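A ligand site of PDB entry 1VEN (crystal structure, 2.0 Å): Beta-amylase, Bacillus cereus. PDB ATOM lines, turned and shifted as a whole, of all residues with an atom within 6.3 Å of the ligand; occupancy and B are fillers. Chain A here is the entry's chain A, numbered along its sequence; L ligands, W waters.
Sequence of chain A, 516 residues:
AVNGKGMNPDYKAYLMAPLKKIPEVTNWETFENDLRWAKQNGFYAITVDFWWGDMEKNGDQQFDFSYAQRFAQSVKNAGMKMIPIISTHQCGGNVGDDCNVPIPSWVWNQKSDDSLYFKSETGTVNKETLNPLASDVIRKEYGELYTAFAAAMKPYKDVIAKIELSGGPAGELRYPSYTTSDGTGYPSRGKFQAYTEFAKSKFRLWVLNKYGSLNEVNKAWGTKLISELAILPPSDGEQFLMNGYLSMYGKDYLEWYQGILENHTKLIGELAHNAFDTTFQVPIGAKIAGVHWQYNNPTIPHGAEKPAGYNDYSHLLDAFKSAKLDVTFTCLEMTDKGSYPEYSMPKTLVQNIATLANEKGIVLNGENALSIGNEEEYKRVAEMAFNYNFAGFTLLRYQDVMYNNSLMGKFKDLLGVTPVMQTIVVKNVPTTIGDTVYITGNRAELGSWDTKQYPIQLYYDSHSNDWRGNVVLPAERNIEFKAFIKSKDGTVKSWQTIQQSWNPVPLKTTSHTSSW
Water W1 bridges O1 of the ligand (2.7 Å) and O of Val 95 (3.2 Å).
Water W2 lies within hydrogen-bond range of NZ of Lys 287 (2.6 Å), O3 of the ligand (2.8 Å) and O of Ala 170 (3.2 Å).
The backbone NH of Asn 94 lies close to the side-chain carboxylate of Asp 97 (3.5 Å).
OD2 of Asp 97 is in hydrogen-bond range of N of Gly 92.
The side-chain carboxylate of Asp 49 sits at hydrogen-bond distance from the side-chain hydroxyl of Ser 87, at 2.7 Å.
The backbone NH (N) of Gly 171 lies close to a ring nitrogen (NE2) of His 89, 3.2 Å away.
The backbone carbonyl oxygen of Ala 17 sits at hydrogen-bond distance from the guanidinium group of Arg 397 (3.0 Å).
The side-chain amino group (NZ) of Lys 287 lies within salt-bridge range of the side-chain carboxylate (OE2) of Glu 367 (3.4 Å).
The side-chain sulfur (SG) of Cys 99 is disulfide-bonded to the side-chain sulfur (SG) of Cys 91, at 2.0 Å.
The side-chain carboxylate (OD1) of Asp 97 is in hydrogen-bond range of an oxygen (O1) of the ligand (2.5 Å).
OD1 of Asp 49 sits at hydrogen-bond distance from O5 of the ligand (2.5 Å).
A ring nitrogen (NE2) of His 89 lies within hydrogen-bond range of an oxygen (O2) of the ligand, 2.8 Å away.
NH2 of Arg 397 sits at hydrogen-bond distance from O4 of the ligand (3.0 Å).
The side-chain sulfur of Met 16 sits at hydrogen-bond distance from an oxygen (O5) of the ligand, at 3.1 Å.
Leu 19 touches the ligand (CD2 to O5, 3.8 Å).
CH2 of Trp 51 touches O2 of the ligand, at 3.3 Å.
Asn 94 touches the ligand.
Ala 170 touches the ligand.
Lys 287 touches the ligand.
Hydrophobic or aromatic side chains that line the ligand: Met 16, Leu 19, Trp 51 and His 89.
Within 4 Å of the ligand: Met 16, Leu 19, Asp 49, Trp 51, His 89, Asn 94, Asp 97, Ala 170, Lys 287 and Arg 397.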
ATOM      1  N   MET A  16     -14.198 -17.829 -13.371  1.00  0.00           N
ATOM      2  CA  MET A  16     -15.500 -17.267 -13.707  1.00  0.00           C
ATOM      3  C   MET A  16     -16.548 -17.730 -12.697  1.00  0.00           C
ATOM      4  O   MET A  16     -16.682 -18.917 -12.423  1.00  0.00           O
ATOM      5  CB  MET A  16     -15.915 -17.695 -15.111  1.00  0.00           C
ATOM      6  CG  MET A  16     -15.661 -16.645 -16.185  1.00  0.00           C
ATOM      7  SD  MET A  16     -17.145 -15.696 -16.614  1.00  0.00           S
ATOM      8  CE  MET A  16     -17.264 -14.523 -15.286  1.00  0.00           C
ATOM      9  N   ALA A  17     -17.270 -16.767 -12.144  1.00  0.00           N
ATOM     10  CA  ALA A  17     -18.328 -17.038 -11.164  1.00  0.00           C
ATOM     11  C   ALA A  17     -19.539 -17.678 -11.847  1.00  0.00           C
ATOM     12  O   ALA A  17     -19.603 -17.751 -13.070  1.00  0.00           O
ATOM     13  CB  ALA A  17     -18.744 -15.716 -10.499  1.00  0.00           C
ATOM     14  N   PRO A  18     -20.507 -18.162 -11.058  1.00  0.00           N
ATOM     15  CA  PRO A  18     -21.701 -18.787 -11.649  1.00  0.00           C
ATOM     16  C   PRO A  18     -22.556 -17.739 -12.381  1.00  0.00           C
ATOM     17  O   PRO A  18     -22.360 -16.533 -12.195  1.00  0.00           O
ATOM     18  CB  PRO A  18     -22.430 -19.351 -10.425  1.00  0.00           C
ATOM     19  CG  PRO A  18     -21.305 -19.600  -9.426  1.00  0.00           C
ATOM     20  CD  PRO A  18     -20.489 -18.351  -9.595  1.00  0.00           C
ATOM     21  N   LEU A  19     -23.504 -18.195 -13.193  1.00  0.00           N
ATOM     22  CA  LEU A  19     -24.388 -17.276 -13.904  1.00  0.00           C
ATOM     23  C   LEU A  19     -25.431 -16.739 -12.926  1.00  0.00           C
ATOM     24  O   LEU A  19     -25.797 -15.561 -12.967  1.00  0.00           O
ATOM     25  CB  LEU A  19     -25.061 -17.982 -15.088  1.00  0.00           C
ATOM     26  CG  LEU A  19     -24.137 -18.360 -16.250  1.00  0.00           C
ATOM     27  CD1 LEU A  19     -24.906 -19.151 -17.288  1.00  0.00           C
ATOM     28  CD2 LEU A  19     -23.535 -17.115 -16.875  1.00  0.00           C
ATOM     29  N   VAL A  48     -16.970 -11.712 -12.678  1.00  0.00           N
ATOM     30  CA  VAL A  48     -18.410 -11.924 -12.512  1.00  0.00           C
ATOM     31  C   VAL A  48     -19.299 -11.015 -13.346  1.00  0.00           C
ATOM     32  O   VAL A  48     -18.980  -9.840 -13.558  1.00  0.00           O
ATOM     33  CB  VAL A  48     -18.781 -11.740 -11.019  1.00  0.00           C
ATOM     34  CG1 VAL A  48     -18.246 -10.396 -10.529  1.00  0.00           C
ATOM     35  CG2 VAL A  48     -20.287 -11.794 -10.832  1.00  0.00           C
ATOM     36  N   ASP A  49     -20.409 -11.570 -13.824  1.00  0.00           N
ATOM     37  CA  ASP A  49     -21.388 -10.808 -14.602  1.00  0.00           C
ATOM     38  C   ASP A  49     -22.303  -9.992 -13.699  1.00  0.00           C
ATOM     39  O   ASP A  49     -22.897 -10.525 -12.760  1.00  0.00           O
ATOM     40  CB  ASP A  49     -22.327 -11.707 -15.418  1.00  0.00           C
ATOM     41  CG  ASP A  49     -21.629 -12.457 -16.522  1.00  0.00           C
ATOM     42  OD1 ASP A  49     -21.174 -13.581 -16.260  1.00  0.00           O
ATOM     43  OD2 ASP A  49     -21.552 -11.910 -17.649  1.00  0.00           O
ATOM     44  N   TRP A  51     -25.496  -8.073 -14.361  1.00  0.00           N
ATOM     45  CA  TRP A  51     -26.529  -7.889 -15.375  1.00  0.00           C
ATOM     46  C   TRP A  51     -27.228  -6.543 -15.378  1.00  0.00           C
ATOM     47  O   TRP A  51     -27.680  -6.053 -14.339  1.00  0.00           O
ATOM     48  CB  TRP A  51     -27.562  -9.014 -15.254  1.00  0.00           C
ATOM     49  CG  TRP A  51     -26.944 -10.356 -15.285  1.00  0.00           C
ATOM     50  CD1 TRP A  51     -26.681 -11.167 -14.207  1.00  0.00           C
ATOM     51  CD2 TRP A  51     -26.365 -11.006 -16.417  1.00  0.00           C
ATOM     52  NE1 TRP A  51     -25.976 -12.276 -14.600  1.00  0.00           N
ATOM     53  CE2 TRP A  51     -25.763 -12.205 -15.962  1.00  0.00           C
ATOM     54  CE3 TRP A  51     -26.300 -10.699 -17.787  1.00  0.00           C
ATOM     55  CZ2 TRP A  51     -25.105 -13.088 -16.820  1.00  0.00           C
ATOM     56  CZ3 TRP A  51     -25.633 -11.579 -18.643  1.00  0.00           C
ATOM     57  CH2 TRP A  51     -25.042 -12.752 -18.155  1.00  0.00           C
ATOM     58  N   ILE A  85     -17.874  -7.714 -14.988  1.00  0.00           N
ATOM     59  CA  ILE A  85     -18.220  -7.639 -16.398  1.00  0.00           C
ATOM     60  C   ILE A  85     -19.527  -6.856 -16.376  1.00  0.00           C
ATOM     61  O   ILE A  85     -20.499  -7.297 -15.761  1.00  0.00           O
ATOM     62  CB  ILE A  85     -18.513  -9.015 -17.019  1.00  0.00           C
ATOM     63  CG1 ILE A  85     -17.322  -9.954 -16.812  1.00  0.00           C
ATOM     64  CG2 ILE A  85     -18.824  -8.853 -18.502  1.00  0.00           C
ATOM     65  CD1 ILE A  85     -17.542 -11.356 -17.355  1.00  0.00           C
ATOM     66  N   SER A  87     -22.320  -6.540 -17.887  1.00  0.00           N
ATOM     67  CA  SER A  87     -23.103  -7.253 -18.890  1.00  0.00           C
ATOM     68  C   SER A  87     -24.399  -6.599 -19.336  1.00  0.00           C
ATOM     69  O   SER A  87     -25.456  -6.809 -18.728  1.00  0.00           O
ATOM     70  CB  SER A  87     -23.374  -8.666 -18.397  1.00  0.00           C
ATOM     71  OG  SER A  87     -22.151  -9.308 -18.089  1.00  0.00           O
ATOM     72  N   HIS A  89     -26.058  -7.334 -21.813  1.00  0.00           N
ATOM     73  CA  HIS A  89     -26.683  -8.279 -22.716  1.00  0.00           C
ATOM     74  C   HIS A  89     -27.567  -9.221 -21.896  1.00  0.00           C
ATOM     75  O   HIS A  89     -27.476  -9.247 -20.670  1.00  0.00           O
ATOM     76  CB  HIS A  89     -25.635  -9.088 -23.506  1.00  0.00           C
ATOM     77  CG  HIS A  89     -24.752  -9.949 -22.641  1.00  0.00           C
ATOM     78  ND1 HIS A  89     -23.655  -9.456 -21.967  1.00  0.00           N
ATOM     79  CD2 HIS A  89     -24.835 -11.261 -22.324  1.00  0.00           C
ATOM     80  CE1 HIS A  89     -23.098 -10.432 -21.276  1.00  0.00           C
ATOM     81  NE2 HIS A  89     -23.791 -11.535 -21.477  1.00  0.00           N
ATOM     82  N   GLN A  90     -28.395 -10.006 -22.573  1.00  0.00           N
ATOM     83  CA  GLN A  90     -29.291 -10.931 -21.892  1.00  0.00           C
ATOM     84  C   GLN A  90     -28.622 -12.226 -21.419  1.00  0.00           C
ATOM     85  O   GLN A  90     -27.768 -12.794 -22.101  1.00  0.00           O
ATOM     86  CB  GLN A  90     -30.457 -11.278 -22.811  1.00  0.00           C
ATOM     87  CG  GLN A  90     -31.319 -12.440 -22.316  1.00  0.00           C
ATOM     88  CD  GLN A  90     -32.494 -12.715 -23.240  1.00  0.00           C
ATOM     89  OE1 GLN A  90     -33.308 -11.833 -23.511  1.00  0.00           O
ATOM     90  NE2 GLN A  90     -32.589 -13.947 -23.735  1.00  0.00           N
ATOM     91  N   CYS A  91     -29.026 -12.673 -20.229  1.00  0.00           N
ATOM     92  CA  CYS A  91     -28.521 -13.929 -19.686  1.00  0.00           C
ATOM     93  C   CYS A  91     -29.634 -14.931 -19.943  1.00  0.00           C
ATOM     94  O   CYS A  91     -30.778 -14.722 -19.524  1.00  0.00           O
ATOM     95  CB  CYS A  91     -28.272 -13.838 -18.180  1.00  0.00           C
ATOM     96  SG  CYS A  91     -27.267 -15.213 -17.515  1.00  0.00           S
ATOM     97  N   GLY A  92     -29.310 -16.026 -20.625  1.00  0.00           N
ATOM     98  CA  GLY A  92     -30.313 -17.037 -20.904  1.00  0.00           C
ATOM     99  C   GLY A  92     -30.602 -17.110 -22.378  1.00  0.00           C
ATOM    100  O   GLY A  92     -30.758 -16.088 -23.037  1.00  0.00           O
ATOM    101  N   ASN A  94     -28.508 -18.716 -24.487  1.00  0.00           N
ATOM    102  CA  ASN A  94     -27.245 -19.090 -25.102  1.00  0.00           C
ATOM    103  C   ASN A  94     -26.768 -20.437 -24.556  1.00  0.00           C
ATOM    104  O   ASN A  94     -27.294 -20.937 -23.550  1.00  0.00           O
ATOM    105  CB  ASN A  94     -26.187 -18.013 -24.828  1.00  0.00           C
ATOM    106  CG  ASN A  94     -26.249 -16.867 -25.826  1.00  0.00           C
ATOM    107  OD1 ASN A  94     -26.034 -15.712 -25.473  1.00  0.00           O
ATOM    108  ND2 ASN A  94     -26.530 -17.195 -27.084  1.00  0.00           N
ATOM    109  N   VAL A  95     -25.781 -21.033 -25.232  1.00  0.00           N
ATOM    110  CA  VAL A  95     -25.241 -22.326 -24.832  1.00  0.00           C
ATOM    111  C   VAL A  95     -24.647 -22.276 -23.428  1.00  0.00           C
ATOM    112  O   VAL A  95     -23.739 -21.481 -23.153  1.00  0.00           O
ATOM    113  CB  VAL A  95     -24.165 -22.820 -25.844  1.00  0.00           C
ATOM    114  CG1 VAL A  95     -23.005 -21.837 -25.896  1.00  0.00           C
ATOM    115  CG2 VAL A  95     -23.662 -24.205 -25.441  1.00  0.00           C
ATOM    116  N   GLY A  96     -25.173 -23.109 -22.532  1.00  0.00           N
ATOM    117  CA  GLY A  96     -24.683 -23.158 -21.167  1.00  0.00           C
ATOM    118  C   GLY A  96     -25.381 -22.208 -20.205  1.00  0.00           C
ATOM    119  O   GLY A  96     -25.110 -22.236 -19.002  1.00  0.00           O
ATOM    120  N   ASP A  97     -26.260 -21.372 -20.735  1.00  0.00           N
ATOM    121  CA  ASP A  97     -26.978 -20.408 -19.913  1.00  0.00           C
ATOM    122  C   ASP A  97     -28.013 -21.070 -18.997  1.00  0.00           C
ATOM    123  O   ASP A  97     -28.885 -21.821 -19.440  1.00  0.00           O
ATOM    124  CB  ASP A  97     -27.661 -19.362 -20.793  1.00  0.00           C
ATOM    125  CG  ASP A  97     -26.697 -18.273 -21.258  1.00  0.00           C
ATOM    126  OD1 ASP A  97     -25.472 -18.490 -21.219  1.00  0.00           O
ATOM    127  OD2 ASP A  97     -27.177 -17.190 -21.670  1.00  0.00           O
ATOM    128  N   CYS A  99     -29.941 -19.180 -16.536  1.00  0.00           N
ATOM    129  CA  CYS A  99     -30.403 -17.923 -15.959  1.00  0.00           C
ATOM    130  C   CYS A  99     -31.454 -17.366 -16.904  1.00  0.00           C
ATOM    131  O   CYS A  99     -31.701 -17.917 -17.979  1.00  0.00           O
ATOM    132  CB  CYS A  99     -29.247 -16.927 -15.911  1.00  0.00           C
ATOM    133  SG  CYS A  99     -28.476 -16.845 -17.559  1.00  0.00           S
ATOM    134  N   PRO A 169     -24.057  -9.977 -27.847  1.00  0.00           N
ATOM    135  CA  PRO A 169     -24.621 -11.234 -27.358  1.00  0.00           C
ATOM    136  C   PRO A 169     -23.605 -11.997 -26.533  1.00  0.00           C
ATOM    137  O   PRO A 169     -22.452 -12.128 -26.945  1.00  0.00           O
ATOM    138  CB  PRO A 169     -24.956 -11.994 -28.643  1.00  0.00           C
ATOM    139  CG  PRO A 169     -25.121 -10.920 -29.654  1.00  0.00           C
ATOM    140  CD  PRO A 169     -24.024  -9.967 -29.318  1.00  0.00           C
ATOM    141  N   ALA A 170     -24.037 -12.513 -25.386  1.00  0.00           N
ATOM    142  CA  ALA A 170     -23.157 -13.290 -24.518  1.00  0.00           C
ATOM    143  C   ALA A 170     -21.905 -12.504 -24.115  1.00  0.00           C
ATOM    144  O   ALA A 170     -20.886 -13.098 -23.786  1.00  0.00           O
ATOM    145  CB  ALA A 170     -22.743 -14.589 -25.218  1.00  0.00           C
ATOM    146  N   GLY A 171     -22.011 -11.182 -24.144  1.00  0.00           N
ATOM    147  CA  GLY A 171     -20.886 -10.341 -23.772  1.00  0.00           C
ATOM    148  C   GLY A 171     -19.739 -10.314 -24.762  1.00  0.00           C
ATOM    149  O   GLY A 171     -18.637  -9.899 -24.423  1.00  0.00           O
ATOM    150  N   LYS A 287     -14.544  -8.719 -25.239  1.00  0.00           N
ATOM    151  CA  LYS A 287     -14.282 -10.059 -25.770  1.00  0.00           C
ATOM    152  C   LYS A 287     -14.642 -10.253 -27.232  1.00  0.00           C
ATOM    153  O   LYS A 287     -15.607  -9.676 -27.734  1.00  0.00           O
ATOM    154  CB  LYS A 287     -15.062 -11.127 -25.012  1.00  0.00           C
ATOM    155  CG  LYS A 287     -14.963 -11.135 -23.500  1.00  0.00           C
ATOM    156  CD  LYS A 287     -15.817 -12.300 -22.982  1.00  0.00           C
ATOM    157  CE  LYS A 287     -15.945 -12.282 -21.469  1.00  0.00           C
ATOM    158  NZ  LYS A 287     -16.773 -13.417 -20.985  1.00  0.00           N
ATOM    159  N   GLU A 367      -9.844 -17.655 -22.569  1.00  0.00           N
ATOM    160  CA  GLU A 367     -10.843 -18.394 -21.797  1.00  0.00           C
ATOM    161  C   GLU A 367     -11.100 -19.705 -22.539  1.00  0.00           C
ATOM    162  O   GLU A 367     -10.758 -19.831 -23.708  1.00  0.00           O
ATOM    163  CB  GLU A 367     -12.198 -17.671 -21.750  1.00  0.00           C
ATOM    164  CG  GLU A 367     -12.215 -16.277 -21.212  1.00  0.00           C
ATOM    165  CD  GLU A 367     -13.641 -15.741 -21.077  1.00  0.00           C
ATOM    166  OE1 GLU A 367     -14.502 -16.086 -21.918  1.00  0.00           O
ATOM    167  OE2 GLU A 367     -13.893 -14.958 -20.136  1.00  0.00           O
ATOM    168  N   LEU A 396     -13.811 -21.080 -17.146  1.00  0.00           N
ATOM    169  CA  LEU A 396     -15.253 -21.210 -17.079  1.00  0.00           C
ATOM    170  C   LEU A 396     -15.413 -22.684 -16.690  1.00  0.00           C
ATOM    171  O   LEU A 396     -14.958 -23.550 -17.439  1.00  0.00           O
ATOM    172  CB  LEU A 396     -15.903 -20.959 -18.447  1.00  0.00           C
ATOM    173  CG  LEU A 396     -16.170 -19.525 -18.946  1.00  0.00           C
ATOM    174  CD1 LEU A 396     -14.860 -18.762 -19.148  1.00  0.00           C
ATOM    175  CD2 LEU A 396     -16.953 -19.603 -20.261  1.00  0.00           C
ATOM    176  N   ARG A 397     -16.046 -22.992 -15.564  1.00  0.00           N
ATOM    177  CA  ARG A 397     -16.628 -22.027 -14.659  1.00  0.00           C
ATOM    178  C   ARG A 397     -16.586 -22.554 -13.219  1.00  0.00           C
ATOM    179  O   ARG A 397     -16.461 -23.758 -12.983  1.00  0.00           O
ATOM    180  CB  ARG A 397     -18.092 -21.783 -15.092  1.00  0.00           C
ATOM    181  CG  ARG A 397     -18.820 -20.682 -14.350  1.00  0.00           C
ATOM    182  CD  ARG A 397     -20.300 -20.609 -14.772  1.00  0.00           C
ATOM    183  NE  ARG A 397     -20.472 -20.333 -16.194  1.00  0.00           N
ATOM    184  CZ  ARG A 397     -20.375 -19.128 -16.756  1.00  0.00           C
ATOM    185  NH1 ARG A 397     -20.101 -18.067 -16.014  1.00  0.00           N
ATOM    186  NH2 ARG A 397     -20.540 -18.994 -18.067  1.00  0.00           N
HETATM  187  C1  LIG L   1     -21.573 -17.186 -21.080  1.00  0.00           C
HETATM  188  C2  LIG L   1     -22.932 -16.504 -20.984  1.00  0.00           C
HETATM  189  C3  LIG L   1     -22.730 -14.983 -20.993  1.00  0.00           C
HETATM  190  C4  LIG L   1     -21.834 -14.584 -19.828  1.00  0.00           C
HETATM  191  C5  LIG L   1     -20.494 -15.339 -19.943  1.00  0.00           C
HETATM  192  C6  LIG L   1     -19.562 -15.068 -18.778  1.00  0.00           C
HETATM  193  O1  LIG L   1     -23.731 -16.897 -22.094  1.00  0.00           O
HETATM  194  O2  LIG L   1     -23.973 -14.304 -20.899  1.00  0.00           O
HETATM  195  O3  LIG L   1     -21.607 -13.186 -19.850  1.00  0.00           O
HETATM  196  O4  LIG L   1     -20.726 -16.766 -19.998  1.00  0.00           O
HETATM  197  O5  LIG L   1     -20.118 -15.510 -17.541  1.00  0.00           O
HETATM  198  O   HOH W   1     -23.140 -18.524 -24.146  1.00  0.00           O
HETATM  199  O   HOH W   2     -19.215 -12.488 -21.179  1.00  0.00           O
HETATM  200  O   HOH W   3     -25.936 -15.068 -22.676  1.00  0.00           O
